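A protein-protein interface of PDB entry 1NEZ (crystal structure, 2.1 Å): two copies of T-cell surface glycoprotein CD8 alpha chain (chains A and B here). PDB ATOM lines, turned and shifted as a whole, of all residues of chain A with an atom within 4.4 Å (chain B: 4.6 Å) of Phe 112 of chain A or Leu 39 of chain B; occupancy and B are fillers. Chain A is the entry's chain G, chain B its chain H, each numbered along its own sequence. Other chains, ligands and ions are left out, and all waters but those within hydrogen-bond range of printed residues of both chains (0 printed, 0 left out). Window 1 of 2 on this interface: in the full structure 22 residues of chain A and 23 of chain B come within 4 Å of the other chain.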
ATOM      1  N   LEU A   7      19.033   0.331 -43.326  1.00  0.00           N
ATOM      2  CA  LEU A   7      20.467   0.499 -43.455  1.00  0.00           C
ATOM      3  C   LEU A   7      21.113  -0.826 -43.829  1.00  0.00           C
ATOM      4  O   LEU A   7      20.987  -1.811 -43.102  1.00  0.00           O
ATOM      5  CB  LEU A   7      21.048   1.032 -42.131  1.00  0.00           C
ATOM      6  CG  LEU A   7      20.934   2.528 -41.780  1.00  0.00           C
ATOM      7  CD1 LEU A   7      19.703   3.129 -42.326  1.00  0.00           C
ATOM      8  CD2 LEU A   7      20.975   2.683 -40.283  1.00  0.00           C
ATOM      9  N   PHE A 101      29.116  -0.565 -36.990  1.00  0.00           N
ATOM     10  CA  PHE A 101      27.766  -0.415 -37.492  1.00  0.00           C
ATOM     11  C   PHE A 101      27.491   1.037 -37.832  1.00  0.00           C
ATOM     12  O   PHE A 101      28.173   1.952 -37.329  1.00  0.00           O
ATOM     13  CB  PHE A 101      26.718  -0.970 -36.501  1.00  0.00           C
ATOM     14  CG  PHE A 101      26.839  -0.448 -35.105  1.00  0.00           C
ATOM     15  CD1 PHE A 101      27.742  -1.011 -34.208  1.00  0.00           C
ATOM     16  CD2 PHE A 101      26.051   0.619 -34.681  1.00  0.00           C
ATOM     17  CE1 PHE A 101      27.859  -0.518 -32.909  1.00  0.00           C
ATOM     18  CE2 PHE A 101      26.160   1.117 -33.394  1.00  0.00           C
ATOM     19  CZ  PHE A 101      27.061   0.556 -32.503  1.00  0.00           C
ATOM     20  N   CYS A 102      26.534   1.256 -38.723  1.00  0.00           N
ATOM     21  CA  CYS A 102      26.192   2.614 -39.097  1.00  0.00           C
ATOM     22  C   CYS A 102      24.839   2.937 -38.492  1.00  0.00           C
ATOM     23  O   CYS A 102      24.107   2.034 -38.074  1.00  0.00           O
ATOM     24  CB  CYS A 102      26.196   2.811 -40.628  1.00  0.00           C
ATOM     25  SG  CYS A 102      25.127   1.673 -41.533  1.00  0.00           S
ATOM     26  N   SER A 103      24.508   4.228 -38.447  1.00  0.00           N
ATOM     27  CA  SER A 103      23.269   4.673 -37.818  1.00  0.00           C
ATOM     28  C   SER A 103      22.657   5.895 -38.501  1.00  0.00           C
ATOM     29  O   SER A 103      23.366   6.730 -39.029  1.00  0.00           O
ATOM     30  CB  SER A 103      23.574   5.017 -36.350  1.00  0.00           C
ATOM     31  OG  SER A 103      22.417   5.386 -35.643  1.00  0.00           O
ATOM     32  N   MET A 110      16.248   6.288 -33.821  1.00  0.00           N
ATOM     33  CA  MET A 110      17.602   5.895 -34.221  1.00  0.00           C
ATOM     34  C   MET A 110      17.497   4.499 -34.841  1.00  0.00           C
ATOM     35  O   MET A 110      16.996   3.574 -34.212  1.00  0.00           O
ATOM     36  CB  MET A 110      18.545   5.787 -33.024  1.00  0.00           C
ATOM     37  CG  MET A 110      18.954   7.102 -32.391  1.00  0.00           C
ATOM     38  SD  MET A 110      20.139   6.811 -31.075  1.00  0.00           S
ATOM     39  CE  MET A 110      21.558   6.242 -32.051  1.00  0.00           C
ATOM     40  N   TYR A 111      17.961   4.361 -36.073  1.00  0.00           N
ATOM     41  CA  TYR A 111      17.960   3.069 -36.765  1.00  0.00           C
ATOM     42  C   TYR A 111      19.418   2.598 -36.901  1.00  0.00           C
ATOM     43  O   TYR A 111      20.306   3.420 -37.179  1.00  0.00           O
ATOM     44  CB  TYR A 111      17.360   3.241 -38.156  1.00  0.00           C
ATOM     45  CG  TYR A 111      15.892   3.619 -38.166  1.00  0.00           C
ATOM     46  CD1 TYR A 111      14.903   2.634 -38.210  1.00  0.00           C
ATOM     47  CD2 TYR A 111      15.493   4.954 -38.116  1.00  0.00           C
ATOM     48  CE1 TYR A 111      13.553   2.973 -38.204  1.00  0.00           C
ATOM     49  CE2 TYR A 111      14.143   5.302 -38.106  1.00  0.00           C
ATOM     50  CZ  TYR A 111      13.185   4.303 -38.149  1.00  0.00           C
ATOM     51  OH  TYR A 111      11.857   4.627 -38.104  1.00  0.00           O
ATOM     52  N   PHE A 112      19.658   1.295 -36.728  1.00  0.00           N
ATOM     53  CA  PHE A 112      21.008   0.711 -36.831  1.00  0.00           C
ATOM     54  C   PHE A 112      21.150  -0.353 -37.936  1.00  0.00           C
ATOM     55  O   PHE A 112      20.204  -1.079 -38.209  1.00  0.00           O
ATOM     56  CB  PHE A 112      21.381   0.050 -35.505  1.00  0.00           C
ATOM     57  CG  PHE A 112      21.341   0.977 -34.351  1.00  0.00           C
ATOM     58  CD1 PHE A 112      20.296   0.924 -33.437  1.00  0.00           C
ATOM     59  CD2 PHE A 112      22.306   1.971 -34.215  1.00  0.00           C
ATOM     60  CE1 PHE A 112      20.199   1.851 -32.398  1.00  0.00           C
ATOM     61  CE2 PHE A 112      22.224   2.910 -33.177  1.00  0.00           C
ATOM     62  CZ  PHE A 112      21.164   2.846 -32.268  1.00  0.00           C
ATOM     63  N   SER A 113      22.325  -0.449 -38.562  1.00  0.00           N
ATOM     64  CA  SER A 113      22.553  -1.480 -39.580  1.00  0.00           C
ATOM     65  C   SER A 113      22.930  -2.733 -38.799  1.00  0.00           C
ATOM     66  O   SER A 113      22.906  -2.709 -37.572  1.00  0.00           O
ATOM     67  CB  SER A 113      23.734  -1.114 -40.483  1.00  0.00           C
ATOM     68  OG  SER A 113      24.948  -1.131 -39.746  1.00  0.00           O
ATOM     69  N   SER A 114      23.270  -3.824 -39.487  1.00  0.00           N
ATOM     70  CA  SER A 114      23.719  -5.019 -38.768  1.00  0.00           C
ATOM     71  C   SER A 114      25.120  -4.675 -38.264  1.00  0.00           C
ATOM     72  O   SER A 114      25.755  -3.747 -38.751  1.00  0.00           O
ATOM     73  CB  SER A 114      23.856  -6.238 -39.692  1.00  0.00           C
ATOM     74  OG  SER A 114      22.669  -6.498 -40.411  1.00  0.00           O
ATOM     75  N   SER B  37      18.043   9.571 -25.761  1.00  0.00           N
ATOM     76  CA  SER B  37      17.578   8.286 -26.283  1.00  0.00           C
ATOM     77  C   SER B  37      18.055   7.142 -25.419  1.00  0.00           C
ATOM     78  O   SER B  37      19.181   7.142 -24.961  1.00  0.00           O
ATOM     79  CB  SER B  37      18.072   8.045 -27.717  1.00  0.00           C
ATOM     80  OG  SER B  37      17.586   9.024 -28.608  1.00  0.00           O
ATOM     81  N   TRP B  38      17.197   6.149 -25.213  1.00  0.00           N
ATOM     82  CA  TRP B  38      17.575   5.010 -24.409  1.00  0.00           C
ATOM     83  C   TRP B  38      17.859   3.863 -25.346  1.00  0.00           C
ATOM     84  O   TRP B  38      17.053   3.565 -26.214  1.00  0.00           O
ATOM     85  CB  TRP B  38      16.454   4.617 -23.448  1.00  0.00           C
ATOM     86  CG  TRP B  38      16.425   5.428 -22.226  1.00  0.00           C
ATOM     87  CD1 TRP B  38      15.642   6.528 -21.987  1.00  0.00           C
ATOM     88  CD2 TRP B  38      17.218   5.232 -21.045  1.00  0.00           C
ATOM     89  NE1 TRP B  38      15.899   7.021 -20.725  1.00  0.00           N
ATOM     90  CE2 TRP B  38      16.859   6.246 -20.128  1.00  0.00           C
ATOM     91  CE3 TRP B  38      18.197   4.301 -20.676  1.00  0.00           C
ATOM     92  CZ2 TRP B  38      17.444   6.354 -18.861  1.00  0.00           C
ATOM     93  CZ3 TRP B  38      18.785   4.412 -19.408  1.00  0.00           C
ATOM     94  CH2 TRP B  38      18.403   5.431 -18.521  1.00  0.00           C
ATOM     95  N   LEU B  39      19.007   3.228 -25.171  1.00  0.00           N
ATOM     96  CA  LEU B  39      19.374   2.110 -26.036  1.00  0.00           C
ATOM     97  C   LEU B  39      19.495   0.814 -25.230  1.00  0.00           C
ATOM     98  O   LEU B  39      19.724   0.833 -24.026  1.00  0.00           O
ATOM     99  CB  LEU B  39      20.690   2.407 -26.770  1.00  0.00           C
ATOM    100  CG  LEU B  39      20.667   3.641 -27.680  1.00  0.00           C
ATOM    101  CD1 LEU B  39      21.961   3.714 -28.486  1.00  0.00           C
ATOM    102  CD2 LEU B  39      19.496   3.548 -28.636  1.00  0.00           C
ATOM    103  N   PHE B  40      19.345  -0.312 -25.915  1.00  0.00           N
ATOM    104  CA  PHE B  40      19.393  -1.601 -25.256  1.00  0.00           C
ATOM    105  C   PHE B  40      20.153  -2.669 -26.065  1.00  0.00           C
ATOM    106  O   PHE B  40      20.027  -2.777 -27.279  1.00  0.00           O
ATOM    107  CB  PHE B  40      17.941  -2.030 -24.952  1.00  0.00           C
ATOM    108  CG  PHE B  40      17.819  -3.388 -24.324  1.00  0.00           C
ATOM    109  CD1 PHE B  40      18.497  -3.691 -23.153  1.00  0.00           C
ATOM    110  CD2 PHE B  40      17.022  -4.365 -24.914  1.00  0.00           C
ATOM    111  CE1 PHE B  40      18.385  -4.962 -22.570  1.00  0.00           C
ATOM    112  CE2 PHE B  40      16.903  -5.641 -24.340  1.00  0.00           C
ATOM    113  CZ  PHE B  40      17.584  -5.939 -23.173  1.00  0.00           C
ATOM    114  N   GLN B  41      20.974  -3.440 -25.375  1.00  0.00           N
ATOM    115  CA  GLN B  41      21.740  -4.499 -26.014  1.00  0.00           C
ATOM    116  C   GLN B  41      21.382  -5.781 -25.263  1.00  0.00           C
ATOM    117  O   GLN B  41      21.768  -5.966 -24.112  1.00  0.00           O
ATOM    118  CB  GLN B  41      23.226  -4.173 -25.899  1.00  0.00           C
ATOM    119  CG  GLN B  41      24.154  -5.052 -26.702  1.00  0.00           C
ATOM    120  CD  GLN B  41      25.327  -4.267 -27.271  1.00  0.00           C
ATOM    121  OE1 GLN B  41      26.371  -4.838 -27.584  1.00  0.00           O
ATOM    122  NE2 GLN B  41      25.155  -2.952 -27.422  1.00  0.00           N
ATOM    123  N   GLN B  49      24.800  -5.789 -30.534  1.00  0.00           N
ATOM    124  CA  GLN B  49      23.815  -5.225 -31.457  1.00  0.00           C
ATOM    125  C   GLN B  49      22.845  -4.312 -30.694  1.00  0.00           C
ATOM    126  O   GLN B  49      21.892  -4.784 -30.081  1.00  0.00           O
ATOM    127  CB  GLN B  49      23.027  -6.338 -32.151  1.00  0.00           C
ATOM    128  CG  GLN B  49      21.876  -5.846 -33.056  1.00  0.00           C
ATOM    129  CD  GLN B  49      22.353  -5.112 -34.305  1.00  0.00           C
ATOM    130  OE1 GLN B  49      23.324  -5.521 -34.950  1.00  0.00           O
ATOM    131  NE2 GLN B  49      21.660  -4.034 -34.662  1.00  0.00           N
ATOM    132  N   PRO B  50      23.075  -2.988 -30.736  1.00  0.00           N
ATOM    133  CA  PRO B  50      22.201  -2.043 -30.035  1.00  0.00           C
ATOM    134  C   PRO B  50      20.779  -1.975 -30.591  1.00  0.00           C
ATOM    135  O   PRO B  50      20.568  -2.129 -31.788  1.00  0.00           O
ATOM    136  CB  PRO B  50      22.941  -0.715 -30.197  1.00  0.00           C
ATOM    137  CG  PRO B  50      23.567  -0.863 -31.536  1.00  0.00           C
ATOM    138  CD  PRO B  50      24.131  -2.264 -31.468  1.00  0.00           C
ATOM    139  N   THR B  51      19.807  -1.758 -29.714  1.00  0.00           N
ATOM    140  CA  THR B  51      18.421  -1.627 -30.146  1.00  0.00           C
ATOM    141  C   THR B  51      17.830  -0.343 -29.553  1.00  0.00           C
ATOM    142  O   THR B  51      17.976  -0.084 -28.352  1.00  0.00           O
ATOM    143  CB  THR B  51      17.557  -2.833 -29.715  1.00  0.00           C
ATOM    144  OG1 THR B  51      17.823  -3.163 -28.347  1.00  0.00           O
ATOM    145  CG2 THR B  51      17.863  -4.026 -30.586  1.00  0.00           C
ATOM    146  N   PHE B  52      17.189   0.463 -30.397  1.00  0.00           N
ATOM    147  CA  PHE B  52      16.579   1.708 -29.940  1.00  0.00           C
ATOM    148  C   PHE B  52      15.370   1.354 -29.072  1.00  0.00           C
ATOM    149  O   PHE B  52      14.520   0.547 -29.456  1.00  0.00           O
ATOM    150  CB  PHE B  52      16.148   2.560 -31.147  1.00  0.00           C
ATOM    151  CG  PHE B  52      15.409   3.854 -30.780  1.00  0.00           C
ATOM    152  CD1 PHE B  52      16.085   4.923 -30.208  1.00  0.00           C
ATOM    153  CD2 PHE B  52      14.053   4.009 -31.072  1.00  0.00           C
ATOM    154  CE1 PHE B  52      15.429   6.134 -29.938  1.00  0.00           C
ATOM    155  CE2 PHE B  52      13.385   5.227 -30.806  1.00  0.00           C
ATOM    156  CZ  PHE B  52      14.070   6.277 -30.246  1.00  0.00           C
ATOM    157  N   VAL B  53      15.307   1.939 -27.882  1.00  0.00           N
ATOM    158  CA  VAL B  53      14.179   1.689 -27.002  1.00  0.00           C
ATOM    159  C   VAL B  53      13.254   2.882 -27.179  1.00  0.00           C
ATOM    160  O   VAL B  53      12.144   2.726 -27.714  1.00  0.00           O
ATOM    161  CB  VAL B  53      14.609   1.556 -25.511  1.00  0.00           C
ATOM    162  CG1 VAL B  53      13.397   1.170 -24.630  1.00  0.00           C
ATOM    163  CG2 VAL B  53      15.680   0.511 -25.384  1.00  0.00           C
ATOM    164  N   TYR B  99      21.810  -5.179 -21.415  1.00  0.00           N
ATOM    165  CA  TYR B  99      22.609  -3.984 -21.177  1.00  0.00           C
ATOM    166  C   TYR B  99      21.911  -2.717 -21.669  1.00  0.00           C
ATOM    167  O   TYR B  99      21.474  -2.637 -22.821  1.00  0.00           O
ATOM    168  CB  TYR B  99      23.996  -4.175 -21.817  1.00  0.00           C
ATOM    169  CG  TYR B  99      24.629  -5.498 -21.396  1.00  0.00           C
ATOM    170  CD1 TYR B  99      24.300  -6.688 -22.055  1.00  0.00           C
ATOM    171  CD2 TYR B  99      25.442  -5.582 -20.255  1.00  0.00           C
ATOM    172  CE1 TYR B  99      24.744  -7.932 -21.585  1.00  0.00           C
ATOM    173  CE2 TYR B  99      25.896  -6.822 -19.772  1.00  0.00           C
ATOM    174  CZ  TYR B  99      25.537  -7.996 -20.442  1.00  0.00           C
ATOM    175  OH  TYR B  99      25.928  -9.237 -19.957  1.00  0.00           O
ATOM    176  N   TYR B 100      21.802  -1.744 -20.772  1.00  0.00           N
ATOM    177  CA  TYR B 100      21.130  -0.479 -21.060  1.00  0.00           C
ATOM    178  C   TYR B 100      22.055   0.704 -20.958  1.00  0.00           C
ATOM    179  O   TYR B 100      22.909   0.738 -20.081  1.00  0.00           O
ATOM    180  CB  TYR B 100      19.983  -0.222 -20.070  1.00  0.00           C
ATOM    181  CG  TYR B 100      18.803  -1.152 -20.212  1.00  0.00           C
ATOM    182  CD1 TYR B 100      18.790  -2.405 -19.594  1.00  0.00           C
ATOM    183  CD2 TYR B 100      17.703  -0.788 -20.989  1.00  0.00           C
ATOM    184  CE1 TYR B 100      17.707  -3.263 -19.747  1.00  0.00           C
ATOM    185  CE2 TYR B 100      16.635  -1.634 -21.153  1.00  0.00           C
ATOM    186  CZ  TYR B 100      16.637  -2.869 -20.528  1.00  0.00           C
ATOM    187  OH  TYR B 100      15.550  -3.686 -20.677  1.00  0.00           O
ATOM    188  N   PHE B 101      21.863   1.679 -21.846  1.00  0.00           N
ATOM    189  CA  PHE B 101      22.644   2.907 -21.830  1.00  0.00           C
ATOM    190  C   PHE B 101      21.881   4.010 -22.567  1.00  0.00           C
ATOM    191  O   PHE B 101      21.088   3.739 -23.482  1.00  0.00           O
ATOM    192  CB  PHE B 101      24.061   2.717 -22.457  1.00  0.00           C
ATOM    193  CG  PHE B 101      24.062   2.081 -23.828  1.00  0.00           C
ATOM    194  CD1 PHE B 101      24.038   0.691 -23.970  1.00  0.00           C
ATOM    195  CD2 PHE B 101      24.156   2.862 -24.974  1.00  0.00           C
ATOM    196  CE1 PHE B 101      24.115   0.094 -25.224  1.00  0.00           C
ATOM    197  CE2 PHE B 101      24.234   2.273 -26.228  1.00  0.00           C
ATOM    198  CZ  PHE B 101      24.214   0.882 -26.357  1.00  0.00           C
ATOM    199  N   SER B 103      21.901   7.837 -24.637  1.00  0.00           N
ATOM    200  CA  SER B 103      22.705   8.520 -25.612  1.00  0.00           C
ATOM    201  C   SER B 103      22.072   9.865 -25.965  1.00  0.00           C
ATOM    202  O   SER B 103      20.836   9.990 -26.037  1.00  0.00           O
ATOM    203  CB  SER B 103      22.818   7.667 -26.883  1.00  0.00           C
ATOM    204  OG  SER B 103      23.391   8.398 -27.954  1.00  0.00           O
ATOM    205  N   PHE B 112      27.480   8.621 -25.438  1.00  0.00           N
ATOM    206  CA  PHE B 112      26.840   7.496 -24.770  1.00  0.00           C
ATOM    207  C   PHE B 112      27.233   7.405 -23.327  1.00  0.00           C
ATOM    208  O   PHE B 112      28.378   7.674 -22.978  1.00  0.00           O
ATOM    209  CB  PHE B 112      27.234   6.180 -25.448  1.00  0.00           C
ATOM    210  CG  PHE B 112      26.896   6.127 -26.907  1.00  0.00           C
ATOM    211  CD1 PHE B 112      25.661   5.675 -27.329  1.00  0.00           C
ATOM    212  CD2 PHE B 112      27.824   6.538 -27.863  1.00  0.00           C
ATOM    213  CE1 PHE B 112      25.342   5.620 -28.679  1.00  0.00           C
ATOM    214  CE2 PHE B 112      27.518   6.492 -29.218  1.00  0.00           C
ATOM    215  CZ  PHE B 112      26.271   6.027 -29.633  1.00  0.00           C
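The side-chain amide nitrogen (NE2) of Gln 49 of chain B sits at hydrogen-bond distance from the backbone carbonyl oxygen (O) of Ser 113 of chain A (3.4 Å).
The side-chain hydroxyl of Ser 113 of chain A sits at hydrogen-bond distance from the backbone NH of Cys 102 of chain A (3.0 Å). The backbone carbonyl oxygen (O) of Phe 101 of chain B is in hydrogen-bond range of the backbone NH (N) of Leu 39 of chain B, at 2.7 Å. OE1 of Gln 41 of chain B sits at hydrogen-bond distance from N of Gln 49 of chain B.
Among the printed residues, merely in contact across the chains: Met 110 of chain A with Phe 52 of chain B (3.3 Å), Phe 112 of chain A with Pro 50 of chain B (3.5 Å), Phe 101 of chain A with Pro 50 of chain B (3.8 Å), Ser 114 of chain A with Gln 49 of chain B (3.9 Å), Phe 112 of chain A with Phe 52 of chain B (3.9 Å) and Phe 112 of chain A with Leu 39 of chain B (3.96 Å).
Of the printed residues of chain B, Phe 112 of chain A touches Leu 39, Pro 50 and Phe 52. Printed residues of chain B within 4 Å of Ser 114 of chain A: Gln 49 (3.9 Å). Of the printed residues of chain A, Gln 49 of chain B touches Ser 113 and Ser 114. Of the printed residues of chain A, Pro 50 of chain B touches Phe 101 (3.8 Å) and Phe 112 (3.5 Å). Tyr 99 of chain B touches none of the printed residues of chain A. Tyr 100 of chain B touches none of the printed residues of chain A. The nearest printed residue of chain A that does not touch Pro 50 of chain B is Ser 113 of chain A (6.2 Å).
Of the 15 printed residues of chain B, 4 touch a printed residue of chain A. Printed residues of chain B that touch a printed residue of chain A: Leu 39, Gln 49, Pro 50 and Phe 52. Hydrophobic or aromatic side chains of chain B that line the printed part of chain A: Leu 39, Pro 50 and Phe 52. Among the printed residues, no Asp or Glu carboxylate lies within 4 Å of a Lys or Arg side-chain nitrogen of the other chain.
3 positions are printed for both chains.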
